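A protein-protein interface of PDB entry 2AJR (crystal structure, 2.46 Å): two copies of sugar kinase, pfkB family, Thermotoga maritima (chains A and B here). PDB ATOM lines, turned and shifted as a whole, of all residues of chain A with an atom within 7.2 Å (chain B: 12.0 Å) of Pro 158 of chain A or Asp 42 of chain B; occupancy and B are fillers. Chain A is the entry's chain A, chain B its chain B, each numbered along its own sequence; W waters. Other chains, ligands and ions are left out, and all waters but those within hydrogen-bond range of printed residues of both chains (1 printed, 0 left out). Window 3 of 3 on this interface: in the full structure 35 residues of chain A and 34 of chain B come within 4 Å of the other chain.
Printed residues of chain B within 4 Å of Phe 123 of chain A: Arg 25 (3.2 Å), Ile 27 (3.8 Å), Ser 44 (3.8 Å) and Thr 46 (3.6 Å). Of chain B, only Asn 41 (3.6 Å), Asp 42 (3.6 Å) and Ser 44 (3.4 Å) come within 4 Å of Pro 124 of chain A. Gly 125 of chain A touches just one residue of chain B: Lys 45. Pro 126 of chain A touches just one residue of chain B: Lys 45 (3.9 Å). Asp 127 of chain A touches just one residue of chain B: Lys 45. Val 128 of chain A touches none of the printed residues of chain B. No residue of chain B comes within 4 Å of Ile 156 of chain A. Of chain B, only Asp 42 (3.7 Å) and Lys 45 (3.6 Å) come within 4 Å of Pro 158 of chain A. No residue of chain B comes within 4 Å of Val 160 of chain A. Of the printed residues of chain A, Arg 25 of chain B touches Phe 123. Of the printed residues of chain A, Asn 41 of chain B touches Pro 124. Of chain A, only Pro 124 (3.6 Å) and Pro 158 (3.7 Å) come within 4 Å of Asp 42 of chain B. Leu 43 of chain B touches none of the printed residues of chain A. Of the printed residues of chain A, Thr 46 of chain B touches Phe 123. The nearest residue of chain B that does not touch Pro 158 of chain A is Leu 43 of chain B (6.2 Å). The nearest residue of chain A that does not touch Asp 42 of chain B is Gly 125 of chain A (4.7 Å).
Printed residues of chain A that touch a printed residue of chain B: Phe 123, Pro 124, Gly 125, Pro 126, Asp 127 and Pro 158.
Phe 123 of chain A touches Arg 25 of chain B (CE1 to NH2, 3.2 Å). CZ of Phe 123 of chain A touches CG1 of Ile 27 of chain B, at 3.8 Å. Phe 123 of chain A touches Ser 44 of chain B (CD2 to O, 3.8 Å). CB of Phe 123 of chain A touches OG1 of Thr 46 of chain B (3.6 Å). Asn 41 of chain B touches Pro 124 of chain A. Pro 124 of chain A touches Asp 42 of chain B (CG to O, 3.6 Å). Pro 124 of chain A touches Ser 44 of chain B (CD to O, 3.4 Å). Pro 126 of chain A touches Lys 45 of chain B (C to NZ, 3.9 Å). Pro 158 of chain A touches Asp 42 of chain B. CG of Pro 158 of chain A touches NZ of Lys 45 of chain B (3.6 Å).
O of Pro 124 of chain A sits at hydrogen-bond distance from ND2 of Asn 20 of chain A (2.9 Å). The backbone NH (N) of Val 128 of chain A is in hydrogen-bond range of the backbone carbonyl oxygen (O) of Pro 158 of chain A, at 3.1 Å. NH2 of Arg 25 of chain B is in hydrogen-bond range of OG1 of Thr 46 of chain B (3.2 Å). The side-chain amide oxygen (OD1) of Asn 41 of chain B sits close to the backbone NH (N) of Leu 43 of chain B. The side-chain amide nitrogen (ND2) of Asn 41 of chain B sits at hydrogen-bond distance from the side-chain hydroxyl (OG) of Ser 44 of chain B. The backbone carbonyl oxygen (O) of Asp 42 of chain B lies within hydrogen-bond range of the side-chain amino group (NZ) of Lys 45 of chain B (2.7 Å).
Water W1 lies within hydrogen-bond range of the backbone NH (N) of Thr 46 of chain B and the backbone NH (N) of Gly 125 of chain A.
No position is printed for both chains. Of the 12 pairs that touch across the chains among the printed residues, none has its exchanged pair printed and touching as well.
The backbone carbonyl oxygen (O) of Gly 125 of chain A is in hydrogen-bond range of the side-chain amino group (NZ) of Lys 45 of chain B (2.7 Å). The side-chain carboxylate (OD1) of Asp 127 of chain A lies within salt-bridge range of the side-chain amino group (NZ) of Lys 45 of chain B (3.1 Å).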
ATOM      1  N   ASN A  20      30.794  21.128   5.869  1.00  0.00           N
ATOM      2  CA  ASN A  20      30.706  20.359   4.626  1.00  0.00           C
ATOM      3  C   ASN A  20      32.080  19.831   4.172  1.00  0.00           C
ATOM      4  O   ASN A  20      32.617  20.266   3.165  1.00  0.00           O
ATOM      5  CB  ASN A  20      30.068  21.234   3.546  1.00  0.00           C
ATOM      6  CG  ASN A  20      29.425  20.417   2.407  1.00  0.00           C
ATOM      7  OD1 ASN A  20      29.353  19.190   2.465  1.00  0.00           O
ATOM      8  ND2 ASN A  20      28.956  21.117   1.363  1.00  0.00           N
ATOM      9  N   PHE A 123      30.686  18.430  -5.297  1.00  0.00           N
ATOM     10  CA  PHE A 123      29.456  17.804  -4.909  1.00  0.00           C
ATOM     11  C   PHE A 123      28.887  18.497  -3.690  1.00  0.00           C
ATOM     12  O   PHE A 123      29.604  19.126  -2.938  1.00  0.00           O
ATOM     13  CB  PHE A 123      29.701  16.295  -4.698  1.00  0.00           C
ATOM     14  CG  PHE A 123      29.678  15.521  -5.998  1.00  0.00           C
ATOM     15  CD1 PHE A 123      30.736  15.610  -6.886  1.00  0.00           C
ATOM     16  CD2 PHE A 123      28.563  14.777  -6.359  1.00  0.00           C
ATOM     17  CE1 PHE A 123      30.702  14.928  -8.090  1.00  0.00           C
ATOM     18  CE2 PHE A 123      28.531  14.087  -7.560  1.00  0.00           C
ATOM     19  CZ  PHE A 123      29.592  14.177  -8.431  1.00  0.00           C
ATOM     20  N   PRO A 124      27.577  18.410  -3.505  1.00  0.00           N
ATOM     21  CA  PRO A 124      26.944  19.265  -2.506  1.00  0.00           C
ATOM     22  C   PRO A 124      27.115  18.815  -1.059  1.00  0.00           C
ATOM     23  O   PRO A 124      27.009  19.641  -0.165  1.00  0.00           O
ATOM     24  CB  PRO A 124      25.468  19.193  -2.902  1.00  0.00           C
ATOM     25  CG  PRO A 124      25.315  17.832  -3.483  1.00  0.00           C
ATOM     26  CD  PRO A 124      26.603  17.542  -4.198  1.00  0.00           C
ATOM     27  N   GLY A 125      27.325  17.522  -0.821  1.00  0.00           N
ATOM     28  CA  GLY A 125      27.362  16.995   0.536  1.00  0.00           C
ATOM     29  C   GLY A 125      26.047  16.354   0.933  1.00  0.00           C
ATOM     30  O   GLY A 125      25.061  16.489   0.232  1.00  0.00           O
ATOM     31  N   PRO A 126      26.020  15.683   2.094  1.00  0.00           N
ATOM     32  CA  PRO A 126      24.825  14.972   2.561  1.00  0.00           C
ATOM     33  C   PRO A 126      23.759  15.902   3.114  1.00  0.00           C
ATOM     34  O   PRO A 126      24.075  16.982   3.581  1.00  0.00           O
ATOM     35  CB  PRO A 126      25.358  14.124   3.709  1.00  0.00           C
ATOM     36  CG  PRO A 126      26.471  14.945   4.256  1.00  0.00           C
ATOM     37  CD  PRO A 126      27.121  15.602   3.074  1.00  0.00           C
ATOM     38  N   ASP A 127      22.509  15.460   3.063  1.00  0.00           N
ATOM     39  CA  ASP A 127      21.434  16.103   3.810  1.00  0.00           C
ATOM     40  C   ASP A 127      21.664  15.902   5.297  1.00  0.00           C
ATOM     41  O   ASP A 127      21.798  14.772   5.755  1.00  0.00           O
ATOM     42  CB  ASP A 127      20.067  15.478   3.481  1.00  0.00           C
ATOM     43  CG  ASP A 127      19.462  15.992   2.194  1.00  0.00           C
ATOM     44  OD1 ASP A 127      20.124  16.736   1.445  1.00  0.00           O
ATOM     45  OD2 ASP A 127      18.303  15.616   1.927  1.00  0.00           O
ATOM     46  N   VAL A 128      21.683  16.994   6.049  1.00  0.00           N
ATOM     47  CA  VAL A 128      21.766  16.924   7.492  1.00  0.00           C
ATOM     48  C   VAL A 128      20.405  17.272   8.079  1.00  0.00           C
ATOM     49  O   VAL A 128      19.763  18.224   7.662  1.00  0.00           O
ATOM     50  CB  VAL A 128      22.844  17.871   7.999  1.00  0.00           C
ATOM     51  CG1 VAL A 128      22.848  17.917   9.515  1.00  0.00           C
ATOM     52  CG2 VAL A 128      24.224  17.438   7.444  1.00  0.00           C
ATOM     53  N   THR A 129      19.962  16.471   9.030  1.00  0.00           N
ATOM     54  CA  THR A 129      18.684  16.682   9.691  1.00  0.00           C
ATOM     55  C   THR A 129      18.815  17.706  10.816  1.00  0.00           C
ATOM     56  O   THR A 129      19.921  18.144  11.152  1.00  0.00           O
ATOM     57  CB  THR A 129      18.171  15.389  10.317  1.00  0.00           C
ATOM     58  OG1 THR A 129      18.969  15.068  11.466  1.00  0.00           O
ATOM     59  CG2 THR A 129      18.203  14.238   9.305  1.00  0.00           C
ATOM     60  N   ILE A 156      28.002  25.114   3.683  1.00  0.00           N
ATOM     61  CA  ILE A 156      27.014  24.459   4.528  1.00  0.00           C
ATOM     62  C   ILE A 156      26.491  23.287   3.710  1.00  0.00           C
ATOM     63  O   ILE A 156      26.322  23.427   2.506  1.00  0.00           O
ATOM     64  CB  ILE A 156      25.820  25.444   4.783  1.00  0.00           C
ATOM     65  CG1 ILE A 156      26.239  26.571   5.715  1.00  0.00           C
ATOM     66  CG2 ILE A 156      24.614  24.753   5.370  1.00  0.00           C
ATOM     67  CD1 ILE A 156      27.279  26.144   6.724  1.00  0.00           C
ATOM     68  N   PRO A 157      26.242  22.127   4.339  1.00  0.00           N
ATOM     69  CA  PRO A 157      25.591  21.068   3.584  1.00  0.00           C
ATOM     70  C   PRO A 157      24.089  21.331   3.488  1.00  0.00           C
ATOM     71  O   PRO A 157      23.558  22.096   4.280  1.00  0.00           O
ATOM     72  CB  PRO A 157      25.868  19.821   4.428  1.00  0.00           C
ATOM     73  CG  PRO A 157      25.926  20.330   5.817  1.00  0.00           C
ATOM     74  CD  PRO A 157      26.534  21.708   5.723  1.00  0.00           C
ATOM     75  N   PRO A 158      23.416  20.736   2.492  1.00  0.00           N
ATOM     76  CA  PRO A 158      21.974  20.881   2.334  1.00  0.00           C
ATOM     77  C   PRO A 158      21.194  20.476   3.580  1.00  0.00           C
ATOM     78  O   PRO A 158      21.571  19.531   4.271  1.00  0.00           O
ATOM     79  CB  PRO A 158      21.629  19.927   1.171  1.00  0.00           C
ATOM     80  CG  PRO A 158      22.861  19.679   0.473  1.00  0.00           C
ATOM     81  CD  PRO A 158      24.011  19.933   1.410  1.00  0.00           C
ATOM     82  N   GLY A 159      20.107  21.191   3.845  1.00  0.00           N
ATOM     83  CA  GLY A 159      19.237  20.893   4.977  1.00  0.00           C
ATOM     84  C   GLY A 159      19.582  21.682   6.226  1.00  0.00           C
ATOM     85  O   GLY A 159      18.854  21.617   7.218  1.00  0.00           O
ATOM     86  N   VAL A 160      20.690  22.414   6.183  1.00  0.00           N
ATOM     87  CA  VAL A 160      21.128  23.205   7.308  1.00  0.00           C
ATOM     88  C   VAL A 160      20.722  24.637   7.056  1.00  0.00           C
ATOM     89  O   VAL A 160      20.920  25.154   5.967  1.00  0.00           O
ATOM     90  CB  VAL A 160      22.632  23.150   7.455  1.00  0.00           C
ATOM     91  CG1 VAL A 160      23.105  24.187   8.479  1.00  0.00           C
ATOM     92  CG2 VAL A 160      23.079  21.750   7.818  1.00  0.00           C
ATOM     93  N   ASN A 161      20.149  25.283   8.065  1.00  0.00           N
ATOM     94  CA  ASN A 161      19.763  26.672   7.917  1.00  0.00           C
ATOM     95  C   ASN A 161      20.994  27.568   7.789  1.00  0.00           C
ATOM     96  O   ASN A 161      21.942  27.461   8.568  1.00  0.00           O
ATOM     97  CB  ASN A 161      18.908  27.130   9.081  1.00  0.00           C
ATOM     98  CG  ASN A 161      18.261  28.469   8.815  1.00  0.00           C
ATOM     99  OD1 ASN A 161      18.926  29.492   8.816  1.00  0.00           O
ATOM    100  ND2 ASN A 161      16.961  28.465   8.571  1.00  0.00           N
ATOM    101  N   ARG B  25      31.906   5.959 -11.010  1.00  0.00           N
ATOM    102  CA  ARG B  25      31.408   7.258 -10.541  1.00  0.00           C
ATOM    103  C   ARG B  25      30.934   8.044 -11.752  1.00  0.00           C
ATOM    104  O   ARG B  25      31.749   8.572 -12.505  1.00  0.00           O
ATOM    105  CB  ARG B  25      32.525   8.028  -9.852  1.00  0.00           C
ATOM    106  CG  ARG B  25      32.102   9.322  -9.191  1.00  0.00           C
ATOM    107  CD  ARG B  25      31.945   9.160  -7.708  1.00  0.00           C
ATOM    108  NE  ARG B  25      31.307  10.332  -7.128  1.00  0.00           N
ATOM    109  CZ  ARG B  25      31.953  11.417  -6.707  1.00  0.00           C
ATOM    110  NH1 ARG B  25      33.278  11.504  -6.795  1.00  0.00           N
ATOM    111  NH2 ARG B  25      31.262  12.425  -6.186  1.00  0.00           N
ATOM    112  N   ILE B  27      28.954  11.167 -13.415  1.00  0.00           N
ATOM    113  CA  ILE B  27      28.719  12.556 -13.078  1.00  0.00           C
ATOM    114  C   ILE B  27      28.077  13.160 -14.291  1.00  0.00           C
ATOM    115  O   ILE B  27      28.609  13.020 -15.388  1.00  0.00           O
ATOM    116  CB  ILE B  27      30.023  13.267 -12.773  1.00  0.00           C
ATOM    117  CG1 ILE B  27      30.776  12.540 -11.644  1.00  0.00           C
ATOM    118  CG2 ILE B  27      29.772  14.704 -12.418  1.00  0.00           C
ATOM    119  CD1 ILE B  27      32.219  13.019 -11.464  1.00  0.00           C
ATOM    120  N   PHE B  28      26.932  13.818 -14.098  1.00  0.00           N
ATOM    121  CA  PHE B  28      26.132  14.368 -15.207  1.00  0.00           C
ATOM    122  C   PHE B  28      26.209  15.867 -15.257  1.00  0.00           C
ATOM    123  O   PHE B  28      25.628  16.534 -14.413  1.00  0.00           O
ATOM    124  CB  PHE B  28      24.686  13.915 -15.053  1.00  0.00           C
ATOM    125  CG  PHE B  28      24.573  12.451 -15.000  1.00  0.00           C
ATOM    126  CD1 PHE B  28      24.917  11.693 -16.116  1.00  0.00           C
ATOM    127  CD2 PHE B  28      24.246  11.805 -13.822  1.00  0.00           C
ATOM    128  CE1 PHE B  28      24.874  10.319 -16.071  1.00  0.00           C
ATOM    129  CE2 PHE B  28      24.195  10.409 -13.772  1.00  0.00           C
ATOM    130  CZ  PHE B  28      24.512   9.670 -14.895  1.00  0.00           C
ATOM    131  N   ILE B  29      26.948  16.377 -16.240  1.00  0.00           N
ATOM    132  CA  ILE B  29      27.162  17.805 -16.419  1.00  0.00           C
ATOM    133  C   ILE B  29      26.895  18.177 -17.873  1.00  0.00           C
ATOM    134  O   ILE B  29      27.564  17.697 -18.774  1.00  0.00           O
ATOM    135  CB  ILE B  29      28.606  18.217 -16.072  1.00  0.00           C
ATOM    136  CG1 ILE B  29      28.951  17.829 -14.628  1.00  0.00           C
ATOM    137  CG2 ILE B  29      28.772  19.706 -16.265  1.00  0.00           C
ATOM    138  CD1 ILE B  29      30.422  18.059 -14.240  1.00  0.00           C
ATOM    139  N   TYR B  38      32.353  23.325 -11.314  1.00  0.00           N
ATOM    140  CA  TYR B  38      30.971  22.907 -11.455  1.00  0.00           C
ATOM    141  C   TYR B  38      30.429  22.535 -10.093  1.00  0.00           C
ATOM    142  O   TYR B  38      30.933  21.608  -9.487  1.00  0.00           O
ATOM    143  CB  TYR B  38      30.896  21.697 -12.362  1.00  0.00           C
ATOM    144  CG  TYR B  38      31.255  22.005 -13.783  1.00  0.00           C
ATOM    145  CD1 TYR B  38      30.286  22.422 -14.682  1.00  0.00           C
ATOM    146  CD2 TYR B  38      32.568  21.897 -14.231  1.00  0.00           C
ATOM    147  CE1 TYR B  38      30.604  22.717 -15.989  1.00  0.00           C
ATOM    148  CE2 TYR B  38      32.901  22.194 -15.542  1.00  0.00           C
ATOM    149  CZ  TYR B  38      31.913  22.611 -16.417  1.00  0.00           C
ATOM    150  OH  TYR B  38      32.208  22.903 -17.728  1.00  0.00           O
ATOM    151  N   ARG B  39      29.445  23.274  -9.590  1.00  0.00           N
ATOM    152  CA  ARG B  39      28.695  22.848  -8.407  1.00  0.00           C
ATOM    153  C   ARG B  39      27.523  21.966  -8.810  1.00  0.00           C
ATOM    154  O   ARG B  39      26.576  22.443  -9.402  1.00  0.00           O
ATOM    155  CB  ARG B  39      28.162  24.044  -7.648  1.00  0.00           C
ATOM    156  CG  ARG B  39      29.217  24.882  -6.992  1.00  0.00           C
ATOM    157  CD  ARG B  39      28.585  26.102  -6.362  1.00  0.00           C
ATOM    158  NE  ARG B  39      29.571  26.920  -5.639  1.00  0.00           N
ATOM    159  CZ  ARG B  39      30.405  27.806  -6.194  1.00  0.00           C
ATOM    160  NH1 ARG B  39      30.397  28.027  -7.513  1.00  0.00           N
ATOM    161  NH2 ARG B  39      31.259  28.483  -5.418  1.00  0.00           N
ATOM    162  N   ILE B  40      27.614  20.678  -8.509  1.00  0.00           N
ATOM    163  CA  ILE B  40      26.530  19.736  -8.711  1.00  0.00           C
ATOM    164  C   ILE B  40      25.350  20.097  -7.805  1.00  0.00           C
ATOM    165  O   ILE B  40      25.543  20.596  -6.690  1.00  0.00           O
ATOM    166  CB  ILE B  40      26.996  18.309  -8.388  1.00  0.00           C
ATOM    167  CG1 ILE B  40      28.126  17.880  -9.349  1.00  0.00           C
ATOM    168  CG2 ILE B  40      25.833  17.303  -8.473  1.00  0.00           C
ATOM    169  CD1 ILE B  40      27.834  18.066 -10.870  1.00  0.00           C
ATOM    170  N   ASN B  41      24.132  19.844  -8.297  1.00  0.00           N
ATOM    171  CA  ASN B  41      22.903  20.241  -7.609  1.00  0.00           C
ATOM    172  C   ASN B  41      22.702  19.415  -6.348  1.00  0.00           C
ATOM    173  O   ASN B  41      23.100  18.261  -6.283  1.00  0.00           O
ATOM    174  CB  ASN B  41      21.681  20.229  -8.573  1.00  0.00           C
ATOM    175  CG  ASN B  41      20.709  19.059  -8.346  1.00  0.00           C
ATOM    176  OD1 ASN B  41      19.623  19.249  -7.772  1.00  0.00           O
ATOM    177  ND2 ASN B  41      21.068  17.865  -8.828  1.00  0.00           N
ATOM    178  N   ASP B  42      22.100  20.028  -5.340  1.00  0.00           N
ATOM    179  CA  ASP B  42      21.993  19.436  -4.016  1.00  0.00           C
ATOM    180  C   ASP B  42      21.458  18.018  -3.940  1.00  0.00           C
ATOM    181  O   ASP B  42      21.777  17.307  -2.985  1.00  0.00           O
ATOM    182  CB  ASP B  42      21.153  20.324  -3.134  1.00  0.00           C
ATOM    183  CG  ASP B  42      21.870  21.597  -2.774  1.00  0.00           C
ATOM    184  OD1 ASP B  42      22.818  21.957  -3.519  1.00  0.00           O
ATOM    185  OD2 ASP B  42      21.491  22.229  -1.761  1.00  0.00           O
ATOM    186  N   LEU B  43      20.681  17.598  -4.941  1.00  0.00           N
ATOM    187  CA  LEU B  43      20.064  16.274  -4.932  1.00  0.00           C
ATOM    188  C   LEU B  43      20.865  15.172  -5.636  1.00  0.00           C
ATOM    189  O   LEU B  43      20.513  13.988  -5.502  1.00  0.00           O
ATOM    190  CB  LEU B  43      18.641  16.328  -5.496  1.00  0.00           C
ATOM    191  CG  LEU B  43      17.518  16.750  -4.543  1.00  0.00           C
ATOM    192  CD1 LEU B  43      17.795  18.065  -3.861  1.00  0.00           C
ATOM    193  CD2 LEU B  43      16.169  16.807  -5.309  1.00  0.00           C
ATOM    194  N   SER B  44      21.910  15.502  -6.391  1.00  0.00           N
ATOM    195  CA  SER B  44      22.775  14.416  -6.876  1.00  0.00           C
ATOM    196  C   SER B  44      23.898  14.234  -5.839  1.00  0.00           C
ATOM    197  O   SER B  44      24.792  15.073  -5.717  1.00  0.00           O
ATOM    198  CB  SER B  44      23.326  14.687  -8.273  1.00  0.00           C
ATOM    199  OG  SER B  44      22.381  15.347  -9.077  1.00  0.00           O
ATOM    200  N   LYS B  45      23.808  13.154  -5.071  1.00  0.00           N
ATOM    201  CA  LYS B  45      24.731  12.851  -3.965  1.00  0.00           C
ATOM    202  C   LYS B  45      25.965  12.052  -4.432  1.00  0.00           C
ATOM    203  O   LYS B  45      25.916  11.354  -5.429  1.00  0.00           O
ATOM    204  CB  LYS B  45      23.975  12.045  -2.908  1.00  0.00           C
ATOM    205  CG  LYS B  45      23.401  12.822  -1.722  1.00  0.00           C
ATOM    206  CD  LYS B  45      22.893  14.219  -1.990  1.00  0.00           C
ATOM    207  CE  LYS B  45      22.276  14.803  -0.718  1.00  0.00           C
ATOM    208  NZ  LYS B  45      22.439  16.267  -0.555  1.00  0.00           N
ATOM    209  N   THR B  46      27.075  12.161  -3.706  1.00  0.00           N
ATOM    210  CA  THR B  46      28.261  11.333  -3.965  1.00  0.00           C
ATOM    211  C   THR B  46      27.860   9.869  -3.869  1.00  0.00           C
ATOM    212  O   THR B  46      27.435   9.397  -2.811  1.00  0.00           O
ATOM    213  CB  THR B  46      29.403  11.654  -2.986  1.00  0.00           C
ATOM    214  OG1 THR B  46      29.904  12.960  -3.286  1.00  0.00           O
ATOM    215  CG2 THR B  46      30.558  10.612  -3.083  1.00  0.00           C
ATOM    216  N   GLN B  47      27.956   9.189  -5.003  1.00  0.00           N
ATOM    217  CA  GLN B  47      27.420   7.848  -5.203  1.00  0.00           C
ATOM    218  C   GLN B  47      28.462   7.038  -5.944  1.00  0.00           C
ATOM    219  O   GLN B  47      29.350   7.580  -6.598  1.00  0.00           O
ATOM    220  CB  GLN B  47      26.152   7.881  -6.077  1.00  0.00           C
ATOM    221  CG  GLN B  47      24.841   8.141  -5.350  1.00  0.00           C
ATOM    222  CD  GLN B  47      23.633   8.111  -6.298  1.00  0.00           C
ATOM    223  OE1 GLN B  47      23.424   7.137  -7.017  1.00  0.00           O
ATOM    224  NE2 GLN B  47      22.841   9.184  -6.298  1.00  0.00           N
HETATM  225  O   HOH W   1      27.483  14.598  -1.981  1.00  0.00           O
